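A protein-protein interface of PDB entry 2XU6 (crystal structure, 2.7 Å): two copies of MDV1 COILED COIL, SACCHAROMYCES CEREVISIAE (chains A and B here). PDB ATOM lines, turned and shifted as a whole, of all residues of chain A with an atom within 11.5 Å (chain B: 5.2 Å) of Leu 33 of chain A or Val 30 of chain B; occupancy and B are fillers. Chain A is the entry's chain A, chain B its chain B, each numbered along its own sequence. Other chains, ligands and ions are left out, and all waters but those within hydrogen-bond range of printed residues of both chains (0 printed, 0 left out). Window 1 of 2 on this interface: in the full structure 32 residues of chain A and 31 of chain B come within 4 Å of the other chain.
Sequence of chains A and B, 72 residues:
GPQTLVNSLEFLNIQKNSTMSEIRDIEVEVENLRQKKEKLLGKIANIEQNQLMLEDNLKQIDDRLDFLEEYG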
ATOM      1  N   ILE A  23      -0.162  -9.692 -17.574  1.00  0.00           N
ATOM      2  CA  ILE A  23      -0.759 -10.795 -16.880  1.00  0.00           C
ATOM      3  C   ILE A  23      -0.011 -11.097 -15.581  1.00  0.00           C
ATOM      4  O   ILE A  23      -0.643 -11.338 -14.562  1.00  0.00           O
ATOM      5  CB  ILE A  23      -0.910 -12.004 -17.777  1.00  0.00           C
ATOM      6  CG1 ILE A  23      -1.984 -11.701 -18.827  1.00  0.00           C
ATOM      7  CG2 ILE A  23      -1.279 -13.235 -16.953  1.00  0.00           C
ATOM      8  CD1 ILE A  23      -2.093 -12.751 -19.918  1.00  0.00           C
ATOM      9  N   ARG A  24       1.318 -11.049 -15.611  1.00  0.00           N
ATOM     10  CA  ARG A  24       2.131 -11.199 -14.409  1.00  0.00           C
ATOM     11  C   ARG A  24       1.910 -10.040 -13.441  1.00  0.00           C
ATOM     12  O   ARG A  24       1.939 -10.223 -12.231  1.00  0.00           O
ATOM     13  CB  ARG A  24       3.600 -11.306 -14.768  1.00  0.00           C
ATOM     14  CG  ARG A  24       4.074 -12.728 -15.045  1.00  0.00           C
ATOM     15  CD  ARG A  24       5.586 -12.780 -15.449  1.00  0.00           C
ATOM     16  NE  ARG A  24       5.794 -12.901 -16.906  1.00  0.00           N
ATOM     17  CZ  ARG A  24       6.081 -11.893 -17.748  1.00  0.00           C
ATOM     18  NH1 ARG A  24       6.219 -10.636 -17.316  1.00  0.00           N
ATOM     19  NH2 ARG A  24       6.228 -12.150 -19.048  1.00  0.00           N
ATOM     20  N   ASP A  25       1.673  -8.852 -13.972  1.00  0.00           N
ATOM     21  CA  ASP A  25       1.325  -7.704 -13.144  1.00  0.00           C
ATOM     22  C   ASP A  25      -0.006  -7.832 -12.402  1.00  0.00           C
ATOM     23  O   ASP A  25      -0.101  -7.488 -11.230  1.00  0.00           O
ATOM     24  CB  ASP A  25       1.282  -6.441 -13.985  1.00  0.00           C
ATOM     25  CG  ASP A  25       2.649  -5.957 -14.360  1.00  0.00           C
ATOM     26  OD1 ASP A  25       3.641  -6.594 -13.924  1.00  0.00           O
ATOM     27  OD2 ASP A  25       2.727  -4.936 -15.085  1.00  0.00           O
ATOM     28  N   ILE A  26      -1.047  -8.272 -13.090  1.00  0.00           N
ATOM     29  CA  ILE A  26      -2.316  -8.489 -12.441  1.00  0.00           C
ATOM     30  C   ILE A  26      -2.101  -9.540 -11.351  1.00  0.00           C
ATOM     31  O   ILE A  26      -2.512  -9.348 -10.213  1.00  0.00           O
ATOM     32  CB  ILE A  26      -3.381  -8.943 -13.458  1.00  0.00           C
ATOM     33  CG1 ILE A  26      -3.726  -7.790 -14.400  1.00  0.00           C
ATOM     34  CG2 ILE A  26      -4.631  -9.464 -12.759  1.00  0.00           C
ATOM     35  CD1 ILE A  26      -4.801  -8.116 -15.449  1.00  0.00           C
ATOM     36  N   GLU A  27      -1.415 -10.629 -11.682  1.00  0.00           N
ATOM     37  CA  GLU A  27      -1.266 -11.732 -10.754  1.00  0.00           C
ATOM     38  C   GLU A  27      -0.600 -11.321  -9.446  1.00  0.00           C
ATOM     39  O   GLU A  27      -0.902 -11.867  -8.395  1.00  0.00           O
ATOM     40  CB  GLU A  27      -0.512 -12.879 -11.396  1.00  0.00           C
ATOM     41  CG  GLU A  27      -1.354 -13.687 -12.335  1.00  0.00           C
ATOM     42  CD  GLU A  27      -0.544 -14.714 -13.104  1.00  0.00           C
ATOM     43  OE1 GLU A  27       0.701 -14.653 -13.077  1.00  0.00           O
ATOM     44  OE2 GLU A  27      -1.146 -15.595 -13.750  1.00  0.00           O
ATOM     45  N   VAL A  28       0.309 -10.362  -9.512  1.00  0.00           N
ATOM     46  CA  VAL A  28       0.933  -9.840  -8.310  1.00  0.00           C
ATOM     47  C   VAL A  28      -0.084  -9.017  -7.526  1.00  0.00           C
ATOM     48  O   VAL A  28      -0.263  -9.249  -6.334  1.00  0.00           O
ATOM     49  CB  VAL A  28       2.195  -9.043  -8.629  1.00  0.00           C
ATOM     50  CG1 VAL A  28       2.650  -8.233  -7.430  1.00  0.00           C
ATOM     51  CG2 VAL A  28       3.277  -9.996  -9.060  1.00  0.00           C
ATOM     52  N   GLU A  29      -0.757  -8.086  -8.196  1.00  0.00           N
ATOM     53  CA  GLU A  29      -1.810  -7.303  -7.580  1.00  0.00           C
ATOM     54  C   GLU A  29      -2.834  -8.185  -6.878  1.00  0.00           C
ATOM     55  O   GLU A  29      -3.322  -7.843  -5.800  1.00  0.00           O
ATOM     56  CB  GLU A  29      -2.526  -6.487  -8.637  1.00  0.00           C
ATOM     57  CG  GLU A  29      -2.163  -5.018  -8.678  1.00  0.00           C
ATOM     58  CD  GLU A  29      -3.388  -4.141  -8.978  1.00  0.00           C
ATOM     59  OE1 GLU A  29      -4.481  -4.436  -8.431  1.00  0.00           O
ATOM     60  OE2 GLU A  29      -3.267  -3.158  -9.755  1.00  0.00           O
ATOM     61  N   VAL A  30      -3.160  -9.320  -7.493  1.00  0.00           N
ATOM     62  CA  VAL A  30      -4.166 -10.214  -6.944  1.00  0.00           C
ATOM     63  C   VAL A  30      -3.615 -10.965  -5.737  1.00  0.00           C
ATOM     64  O   VAL A  30      -4.327 -11.215  -4.787  1.00  0.00           O
ATOM     65  CB  VAL A  30      -4.724 -11.167  -8.011  1.00  0.00           C
ATOM     66  CG1 VAL A  30      -5.676 -12.194  -7.400  1.00  0.00           C
ATOM     67  CG2 VAL A  30      -5.450 -10.368  -9.069  1.00  0.00           C
ATOM     68  N   GLU A  31      -2.341 -11.300  -5.761  1.00  0.00           N
ATOM     69  CA  GLU A  31      -1.735 -11.940  -4.621  1.00  0.00           C
ATOM     70  C   GLU A  31      -1.833 -11.019  -3.406  1.00  0.00           C
ATOM     71  O   GLU A  31      -2.219 -11.450  -2.323  1.00  0.00           O
ATOM     72  CB  GLU A  31      -0.288 -12.309  -4.933  1.00  0.00           C
ATOM     73  CG  GLU A  31       0.396 -13.273  -3.931  1.00  0.00           C
ATOM     74  CD  GLU A  31      -0.527 -14.355  -3.369  1.00  0.00           C
ATOM     75  OE1 GLU A  31      -1.407 -14.854  -4.120  1.00  0.00           O
ATOM     76  OE2 GLU A  31      -0.375 -14.704  -2.164  1.00  0.00           O
ATOM     77  N   ASN A  32      -1.526  -9.743  -3.613  1.00  0.00           N
ATOM     78  CA  ASN A  32      -1.549  -8.758  -2.554  1.00  0.00           C
ATOM     79  C   ASN A  32      -2.910  -8.601  -1.987  1.00  0.00           C
ATOM     80  O   ASN A  32      -3.034  -8.521  -0.788  1.00  0.00           O
ATOM     81  CB  ASN A  32      -1.044  -7.409  -3.035  1.00  0.00           C
ATOM     82  CG  ASN A  32       0.343  -7.499  -3.621  1.00  0.00           C
ATOM     83  OD1 ASN A  32       1.163  -8.311  -3.177  1.00  0.00           O
ATOM     84  ND2 ASN A  32       0.612  -6.689  -4.654  1.00  0.00           N
ATOM     85  N   LEU A  33      -3.935  -8.555  -2.824  1.00  0.00           N
ATOM     86  CA  LEU A  33      -5.295  -8.433  -2.301  1.00  0.00           C
ATOM     87  C   LEU A  33      -5.733  -9.686  -1.546  1.00  0.00           C
ATOM     88  O   LEU A  33      -6.604  -9.625  -0.682  1.00  0.00           O
ATOM     89  CB  LEU A  33      -6.306  -8.085  -3.394  1.00  0.00           C
ATOM     90  CG  LEU A  33      -6.097  -6.751  -4.126  1.00  0.00           C
ATOM     91  CD1 LEU A  33      -7.096  -6.646  -5.255  1.00  0.00           C
ATOM     92  CD2 LEU A  33      -6.151  -5.515  -3.215  1.00  0.00           C
ATOM     93  N   ARG A  34      -5.128 -10.822  -1.854  1.00  0.00           N
ATOM     94  CA  ARG A  34      -5.480 -12.012  -1.152  1.00  0.00           C
ATOM     95  C   ARG A  34      -4.875 -12.026   0.219  1.00  0.00           C
ATOM     96  O   ARG A  34      -5.562 -12.305   1.180  1.00  0.00           O
ATOM     97  CB  ARG A  34      -5.143 -13.242  -1.951  1.00  0.00           C
ATOM     98  CG  ARG A  34      -6.268 -13.514  -2.875  1.00  0.00           C
ATOM     99  CD  ARG A  34      -6.130 -14.797  -3.591  1.00  0.00           C
ATOM    100  NE  ARG A  34      -6.818 -14.680  -4.866  1.00  0.00           N
ATOM    101  CZ  ARG A  34      -7.034 -15.693  -5.699  1.00  0.00           C
ATOM    102  NH1 ARG A  34      -6.631 -16.929  -5.381  1.00  0.00           N
ATOM    103  NH2 ARG A  34      -7.662 -15.475  -6.855  1.00  0.00           N
ATOM    104  N   GLN A  35      -3.603 -11.694   0.313  1.00  0.00           N
ATOM    105  CA  GLN A  35      -2.966 -11.536   1.589  1.00  0.00           C
ATOM    106  C   GLN A  35      -3.662 -10.480   2.438  1.00  0.00           C
ATOM    107  O   GLN A  35      -3.644 -10.565   3.664  1.00  0.00           O
ATOM    108  CB  GLN A  35      -1.543 -11.081   1.398  1.00  0.00           C
ATOM    109  CG  GLN A  35      -0.613 -12.115   0.852  1.00  0.00           C
ATOM    110  CD  GLN A  35       0.666 -11.480   0.291  1.00  0.00           C
ATOM    111  OE1 GLN A  35       0.997 -10.311   0.582  1.00  0.00           O
ATOM    112  NE2 GLN A  35       1.384 -12.249  -0.532  1.00  0.00           N
ATOM    113  N   LYS A  36      -4.253  -9.474   1.801  1.00  0.00           N
ATOM    114  CA  LYS A  36      -4.911  -8.403   2.524  1.00  0.00           C
ATOM    115  C   LYS A  36      -6.216  -8.943   3.086  1.00  0.00           C
ATOM    116  O   LYS A  36      -6.595  -8.644   4.208  1.00  0.00           O
ATOM    117  CB  LYS A  36      -5.213  -7.245   1.588  1.00  0.00           C
ATOM    118  CG  LYS A  36      -4.561  -5.970   2.015  1.00  0.00           C
ATOM    119  CD  LYS A  36      -5.568  -4.829   2.098  1.00  0.00           C
ATOM    120  CE  LYS A  36      -5.286  -3.953   3.342  1.00  0.00           C
ATOM    121  NZ  LYS A  36      -6.560  -3.492   4.003  1.00  0.00           N
ATOM    122  N   LYS A  37      -6.902  -9.751   2.289  1.00  0.00           N
ATOM    123  CA  LYS A  37      -8.163 -10.308   2.685  1.00  0.00           C
ATOM    124  C   LYS A  37      -7.917 -11.379   3.748  1.00  0.00           C
ATOM    125  O   LYS A  37      -8.760 -11.577   4.631  1.00  0.00           O
ATOM    126  CB  LYS A  37      -8.865 -10.878   1.460  1.00  0.00           C
ATOM    127  CG  LYS A  37     -10.293 -11.330   1.668  1.00  0.00           C
ATOM    128  CD  LYS A  37     -10.689 -12.358   0.592  1.00  0.00           C
ATOM    129  CE  LYS A  37     -12.185 -12.643   0.630  1.00  0.00           C
ATOM    130  NZ  LYS A  37     -12.613 -13.844  -0.128  1.00  0.00           N
ATOM    131  N   GLU A  38      -6.782 -12.071   3.673  1.00  0.00           N
ATOM    132  CA  GLU A  38      -6.464 -13.081   4.671  1.00  0.00           C
ATOM    133  C   GLU A  38      -6.341 -12.386   6.019  1.00  0.00           C
ATOM    134  O   GLU A  38      -6.989 -12.795   6.999  1.00  0.00           O
ATOM    135  CB  GLU A  38      -5.173 -13.841   4.342  1.00  0.00           C
ATOM    136  CG  GLU A  38      -5.261 -14.869   3.200  1.00  0.00           C
ATOM    137  CD  GLU A  38      -6.530 -15.688   3.224  1.00  0.00           C
ATOM    138  OE1 GLU A  38      -6.450 -16.929   3.360  1.00  0.00           O
ATOM    139  OE2 GLU A  38      -7.610 -15.081   3.105  1.00  0.00           O
ATOM    140  N   LYS A  39      -5.549 -11.318   6.070  1.00  0.00           N
ATOM    141  CA  LYS A  39      -5.396 -10.583   7.302  1.00  0.00           C
ATOM    142  C   LYS A  39      -6.712 -10.057   7.829  1.00  0.00           C
ATOM    143  O   LYS A  39      -7.006 -10.148   9.012  1.00  0.00           O
ATOM    144  CB  LYS A  39      -4.388  -9.469   7.136  1.00  0.00           C
ATOM    145  CG  LYS A  39      -2.986  -9.968   7.359  1.00  0.00           C
ATOM    146  CD  LYS A  39      -1.979  -9.335   6.403  1.00  0.00           C
ATOM    147  CE  LYS A  39      -0.614 -10.097   6.454  1.00  0.00           C
ATOM    148  NZ  LYS A  39       0.070 -10.176   5.104  1.00  0.00           N
ATOM    149  N   LEU A  40      -7.530  -9.516   6.958  1.00  0.00           N
ATOM    150  CA  LEU A  40      -8.792  -8.967   7.395  1.00  0.00           C
ATOM    151  C   LEU A  40      -9.681 -10.041   7.971  1.00  0.00           C
ATOM    152  O   LEU A  40     -10.487  -9.776   8.854  1.00  0.00           O
ATOM    153  CB  LEU A  40      -9.487  -8.264   6.230  1.00  0.00           C
ATOM    154  CG  LEU A  40      -8.991  -6.841   5.978  1.00  0.00           C
ATOM    155  CD1 LEU A  40      -9.243  -6.470   4.532  1.00  0.00           C
ATOM    156  CD2 LEU A  40      -9.688  -5.886   6.908  1.00  0.00           C
ATOM    157  N   LEU A  41      -9.551 -11.259   7.460  1.00  0.00           N
ATOM    158  CA  LEU A  41     -10.384 -12.353   7.929  1.00  0.00           C
ATOM    159  C   LEU A  41      -9.881 -12.817   9.296  1.00  0.00           C
ATOM    160  O   LEU A  41     -10.671 -13.176  10.165  1.00  0.00           O
ATOM    161  CB  LEU A  41     -10.407 -13.478   6.908  1.00  0.00           C
ATOM    162  CG  LEU A  41     -11.488 -13.408   5.837  1.00  0.00           C
ATOM    163  CD1 LEU A  41     -11.334 -14.619   4.952  1.00  0.00           C
ATOM    164  CD2 LEU A  41     -12.892 -13.381   6.438  1.00  0.00           C
ATOM    165  N   GLY A  42      -8.567 -12.767   9.483  1.00  0.00           N
ATOM    166  CA  GLY A  42      -7.977 -12.893  10.804  1.00  0.00           C
ATOM    167  C   GLY A  42      -8.636 -11.949  11.805  1.00  0.00           C
ATOM    168  O   GLY A  42      -9.028 -12.356  12.916  1.00  0.00           O
ATOM    169  N   ILE B  26     -12.721  -5.919  -1.410  1.00  0.00           N
ATOM    170  CA  ILE B  26     -11.555  -6.644  -1.923  1.00  0.00           C
ATOM    171  C   ILE B  26     -11.971  -7.726  -2.909  1.00  0.00           C
ATOM    172  O   ILE B  26     -11.374  -7.880  -3.952  1.00  0.00           O
ATOM    173  CB  ILE B  26     -10.661  -7.202  -0.806  1.00  0.00           C
ATOM    174  CG1 ILE B  26     -10.017  -6.040  -0.051  1.00  0.00           C
ATOM    175  CG2 ILE B  26      -9.564  -8.064  -1.387  1.00  0.00           C
ATOM    176  CD1 ILE B  26      -8.736  -6.400   0.722  1.00  0.00           C
ATOM    177  N   GLU B  27     -13.033  -8.435  -2.596  1.00  0.00           N
ATOM    178  CA  GLU B  27     -13.505  -9.480  -3.464  1.00  0.00           C
ATOM    179  C   GLU B  27     -13.922  -8.927  -4.813  1.00  0.00           C
ATOM    180  O   GLU B  27     -13.837  -9.616  -5.818  1.00  0.00           O
ATOM    181  CB  GLU B  27     -14.663 -10.206  -2.806  1.00  0.00           C
ATOM    182  CG  GLU B  27     -14.205 -11.121  -1.710  1.00  0.00           C
ATOM    183  CD  GLU B  27     -15.347 -11.651  -0.874  1.00  0.00           C
ATOM    184  OE1 GLU B  27     -16.439 -11.029  -0.892  1.00  0.00           O
ATOM    185  OE2 GLU B  27     -15.144 -12.688  -0.192  1.00  0.00           O
ATOM    186  N   VAL B  28     -14.364  -7.680  -4.831  1.00  0.00           N
ATOM    187  CA  VAL B  28     -14.738  -7.024  -6.068  1.00  0.00           C
ATOM    188  C   VAL B  28     -13.507  -6.680  -6.904  1.00  0.00           C
ATOM    189  O   VAL B  28     -13.378  -7.219  -7.991  1.00  0.00           O
ATOM    190  CB  VAL B  28     -15.724  -5.840  -5.828  1.00  0.00           C
ATOM    191  CG1 VAL B  28     -15.360  -4.621  -6.676  1.00  0.00           C
ATOM    192  CG2 VAL B  28     -17.194  -6.293  -6.069  1.00  0.00           C
ATOM    193  N   GLU B  29     -12.585  -5.850  -6.407  1.00  0.00           N
ATOM    194  CA  GLU B  29     -11.287  -5.674  -7.093  1.00  0.00           C
ATOM    195  C   GLU B  29     -10.736  -6.975  -7.679  1.00  0.00           C
ATOM    196  O   GLU B  29     -10.297  -6.993  -8.815  1.00  0.00           O
ATOM    197  CB  GLU B  29     -10.211  -5.157  -6.160  1.00  0.00           C
ATOM    198  CG  GLU B  29     -10.363  -3.753  -5.663  1.00  0.00           C
ATOM    199  CD  GLU B  29      -9.012  -3.188  -5.218  1.00  0.00           C
ATOM    200  OE1 GLU B  29      -8.009  -3.543  -5.871  1.00  0.00           O
ATOM    201  OE2 GLU B  29      -8.930  -2.406  -4.227  1.00  0.00           O
ATOM    202  N   VAL B  30     -10.739  -8.054  -6.898  1.00  0.00           N
ATOM    203  CA  VAL B  30     -10.157  -9.312  -7.341  1.00  0.00           C
ATOM    204  C   VAL B  30     -10.903  -9.827  -8.563  1.00  0.00           C
ATOM    205  O   VAL B  30     -10.291 -10.192  -9.556  1.00  0.00           O
ATOM    206  CB  VAL B  30     -10.101 -10.376  -6.219  1.00  0.00           C
ATOM    207  CG1 VAL B  30      -9.804 -11.750  -6.769  1.00  0.00           C
ATOM    208  CG2 VAL B  30      -9.025 -10.021  -5.229  1.00  0.00           C
ATOM    209  N   GLU B  31     -12.224  -9.827  -8.491  1.00  0.00           N
ATOM    210  CA  GLU B  31     -13.065 -10.285  -9.575  1.00  0.00           C
ATOM    211  C   GLU B  31     -12.843  -9.452 -10.835  1.00  0.00           C
ATOM    212  O   GLU B  31     -12.767  -9.989 -11.952  1.00  0.00           O
ATOM    213  CB  GLU B  31     -14.527 -10.201  -9.148  1.00  0.00           C
ATOM    214  CG  GLU B  31     -15.507 -10.479 -10.248  1.00  0.00           C
ATOM    215  CD  GLU B  31     -15.239 -11.803 -10.942  1.00  0.00           C
ATOM    216  OE1 GLU B  31     -14.415 -12.621 -10.447  1.00  0.00           O
ATOM    217  OE2 GLU B  31     -15.863 -12.025 -12.002  1.00  0.00           O
ATOM    218  N   ASN B  32     -12.738  -8.140 -10.655  1.00  0.00           N
ATOM    219  CA  ASN B  32     -12.546  -7.280 -11.801  1.00  0.00           C
ATOM    220  C   ASN B  32     -11.122  -7.411 -12.352  1.00  0.00           C
ATOM    221  O   ASN B  32     -10.892  -7.213 -13.545  1.00  0.00           O
ATOM    222  CB  ASN B  32     -13.019  -5.833 -11.531  1.00  0.00           C
ATOM    223  CG  ASN B  32     -11.880  -4.856 -11.273  1.00  0.00           C
ATOM    224  OD1 ASN B  32     -10.943  -4.732 -12.072  1.00  0.00           O
ATOM    225  ND2 ASN B  32     -11.984  -4.119 -10.165  1.00  0.00           N
ATOM    226  N   LEU B  33     -10.171  -7.780 -11.505  1.00  0.00           N
ATOM    227  CA  LEU B  33      -8.841  -8.023 -12.010  1.00  0.00           C
ATOM    228  C   LEU B  33      -8.845  -9.346 -12.697  1.00  0.00           C
ATOM    229  O   LEU B  33      -8.146  -9.523 -13.677  1.00  0.00           O
ATOM    230  CB  LEU B  33      -7.805  -8.035 -10.904  1.00  0.00           C
ATOM    231  CG  LEU B  33      -7.277  -6.688 -10.434  1.00  0.00           C
ATOM    232  CD1 LEU B  33      -5.895  -6.947  -9.927  1.00  0.00           C
ATOM    233  CD2 LEU B  33      -7.236  -5.626 -11.537  1.00  0.00           C
ATOM    234  N   ARG B  34      -9.640 -10.277 -12.195  1.00  0.00           N
ATOM    235  CA  ARG B  34      -9.590 -11.633 -12.710  1.00  0.00           C
ATOM    236  C   ARG B  34     -10.120 -11.672 -14.130  1.00  0.00           C
ATOM    237  O   ARG B  34      -9.780 -12.576 -14.922  1.00  0.00           O
ATOM    238  CB  ARG B  34     -10.395 -12.598 -11.842  1.00  0.00           C
ATOM    239  CG  ARG B  34      -9.890 -14.051 -11.896  1.00  0.00           C
ATOM    240  CD  ARG B  34      -8.712 -14.245 -10.903  1.00  0.00           C
ATOM    241  NE  ARG B  34      -9.021 -15.027  -9.689  1.00  0.00           N
ATOM    242  CZ  ARG B  34     -10.073 -14.856  -8.874  1.00  0.00           C
ATOM    243  NH1 ARG B  34     -11.009 -13.934  -9.107  1.00  0.00           N
ATOM    244  NH2 ARG B  34     -10.203 -15.643  -7.808  1.00  0.00           N
ATOM    245  N   GLN B  35     -10.972 -10.694 -14.437  1.00  0.00           N
ATOM    246  CA  GLN B  35     -11.574 -10.646 -15.742  1.00  0.00           C
ATOM    247  C   GLN B  35     -10.579  -9.991 -16.670  1.00  0.00           C
ATOM    248  O   GLN B  35     -10.257 -10.559 -17.712  1.00  0.00           O
ATOM    249  CB  GLN B  35     -12.959  -9.993 -15.731  1.00  0.00           C
ATOM    250  CG  GLN B  35     -12.974  -8.507 -15.431  1.00  0.00           C
ATOM    251  CD  GLN B  35     -14.314  -8.020 -14.850  1.00  0.00           C
ATOM    252  OE1 GLN B  35     -15.180  -8.828 -14.472  1.00  0.00           O
ATOM    253  NE2 GLN B  35     -14.479  -6.690 -14.759  1.00  0.00           N
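The side-chain carboxylate of Glu 27 of chain B is in salt-bridge range of the side-chain amino group of Lys 37 of chain A (2.8 Å).
The guanidinium group of Arg 34 of chain B sits close to the guanidinium group of Arg 34 of chain A.
The side-chain carboxylate (OE1) of Glu 31 of chain B lies within salt-bridge range of the guanidinium group (NH1) of Arg 34 of chain B, at 3.9 Å.
Ile 26 of chain A touches Leu 33 of chain B (CG2 to O, 3.6 Å).
OE1 of Glu 29 of chain A touches CD1 of Leu 33 of chain B, 3.2 Å away.
Leu 33 of chain B touches Val 30 of chain A.
O of Leu 33 of chain A touches CG2 of Ile 26 of chain B, 3.4 Å away.
Leu 33 of chain A touches Glu 29 of chain B (CD1 to OE1, 3.3 Å).
CB of Leu 33 of chain A touches CG2 of Val 30 of chain B, 3.8 Å away.
Lys 36 of chain A touches Ile 26 of chain B.
Leu 40 of chain A touches Ile 26 of chain B (CD1 to CD1, 3.8 Å).
Leu 33 of chain A touches three residues of chain B.
Val 30 of chain B touches just one residue of chain A: Leu 33.
Glu 29 of chain B touches just one residue of chain A: Leu 33.
Of chain A, only Ile 26, Glu 29 and Val 30 come within 4 Å of Leu 33 of chain B.
Printed residues of chain A within 4 Å of Arg 34 of chain B: Arg 34 (2.7 Å).
Printed residues of chain B within 4 Å of Leu 40 of chain A: Ile 26 (3.8 Å).
Printed residues of chain A within 4 Å of Glu 27 of chain B: Lys 37.
Ile 23 of chain A touches none of the printed residues of chain B.
Gln 35 of chain B touches none of the printed residues of chain A.
The nearest printed residue of chain B that does not touch Ile 26 of chain A is Arg 34 of chain B (5.1 Å).
Of the 20 printed residues of chain A, 8 touch a printed residue of chain B.
Hydrophobic or aromatic side chains of chain A that line the printed part of chain B: Ile 26, Val 30, Leu 33 and Leu 40.
Printed residues of chain B that touch a printed residue of chain A: Ile 26, Glu 27, Glu 29, Val 30, Leu 33 and Arg 34.
Among the printed residues, Asp or Glu carboxylates within 4 Å of a Lys or Arg side-chain nitrogen of the other chain: Lys 37 of chain A with Glu 27 of chain B.
Ile 26 of chain A touches Leu 33 of chain B, and with the chains exchanged Leu 33 of chain A touches Ile 26 of chain B.
Glu 29 of chain A touches Leu 33 of chain B, and with the chains exchanged Leu 33 of chain A touches Glu 29 of chain B.
Val 30 of chain A touches Leu 33 of chain B, and with the chains exchanged Leu 33 of chain A touches Val 30 of chain B.
Arg 34 of chain A touches its own counterpart, Arg 34 of chain B.
Of the 10 pairs that touch across the chains among the printed residues, 7 have their exchanged pair printed and touching as well.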
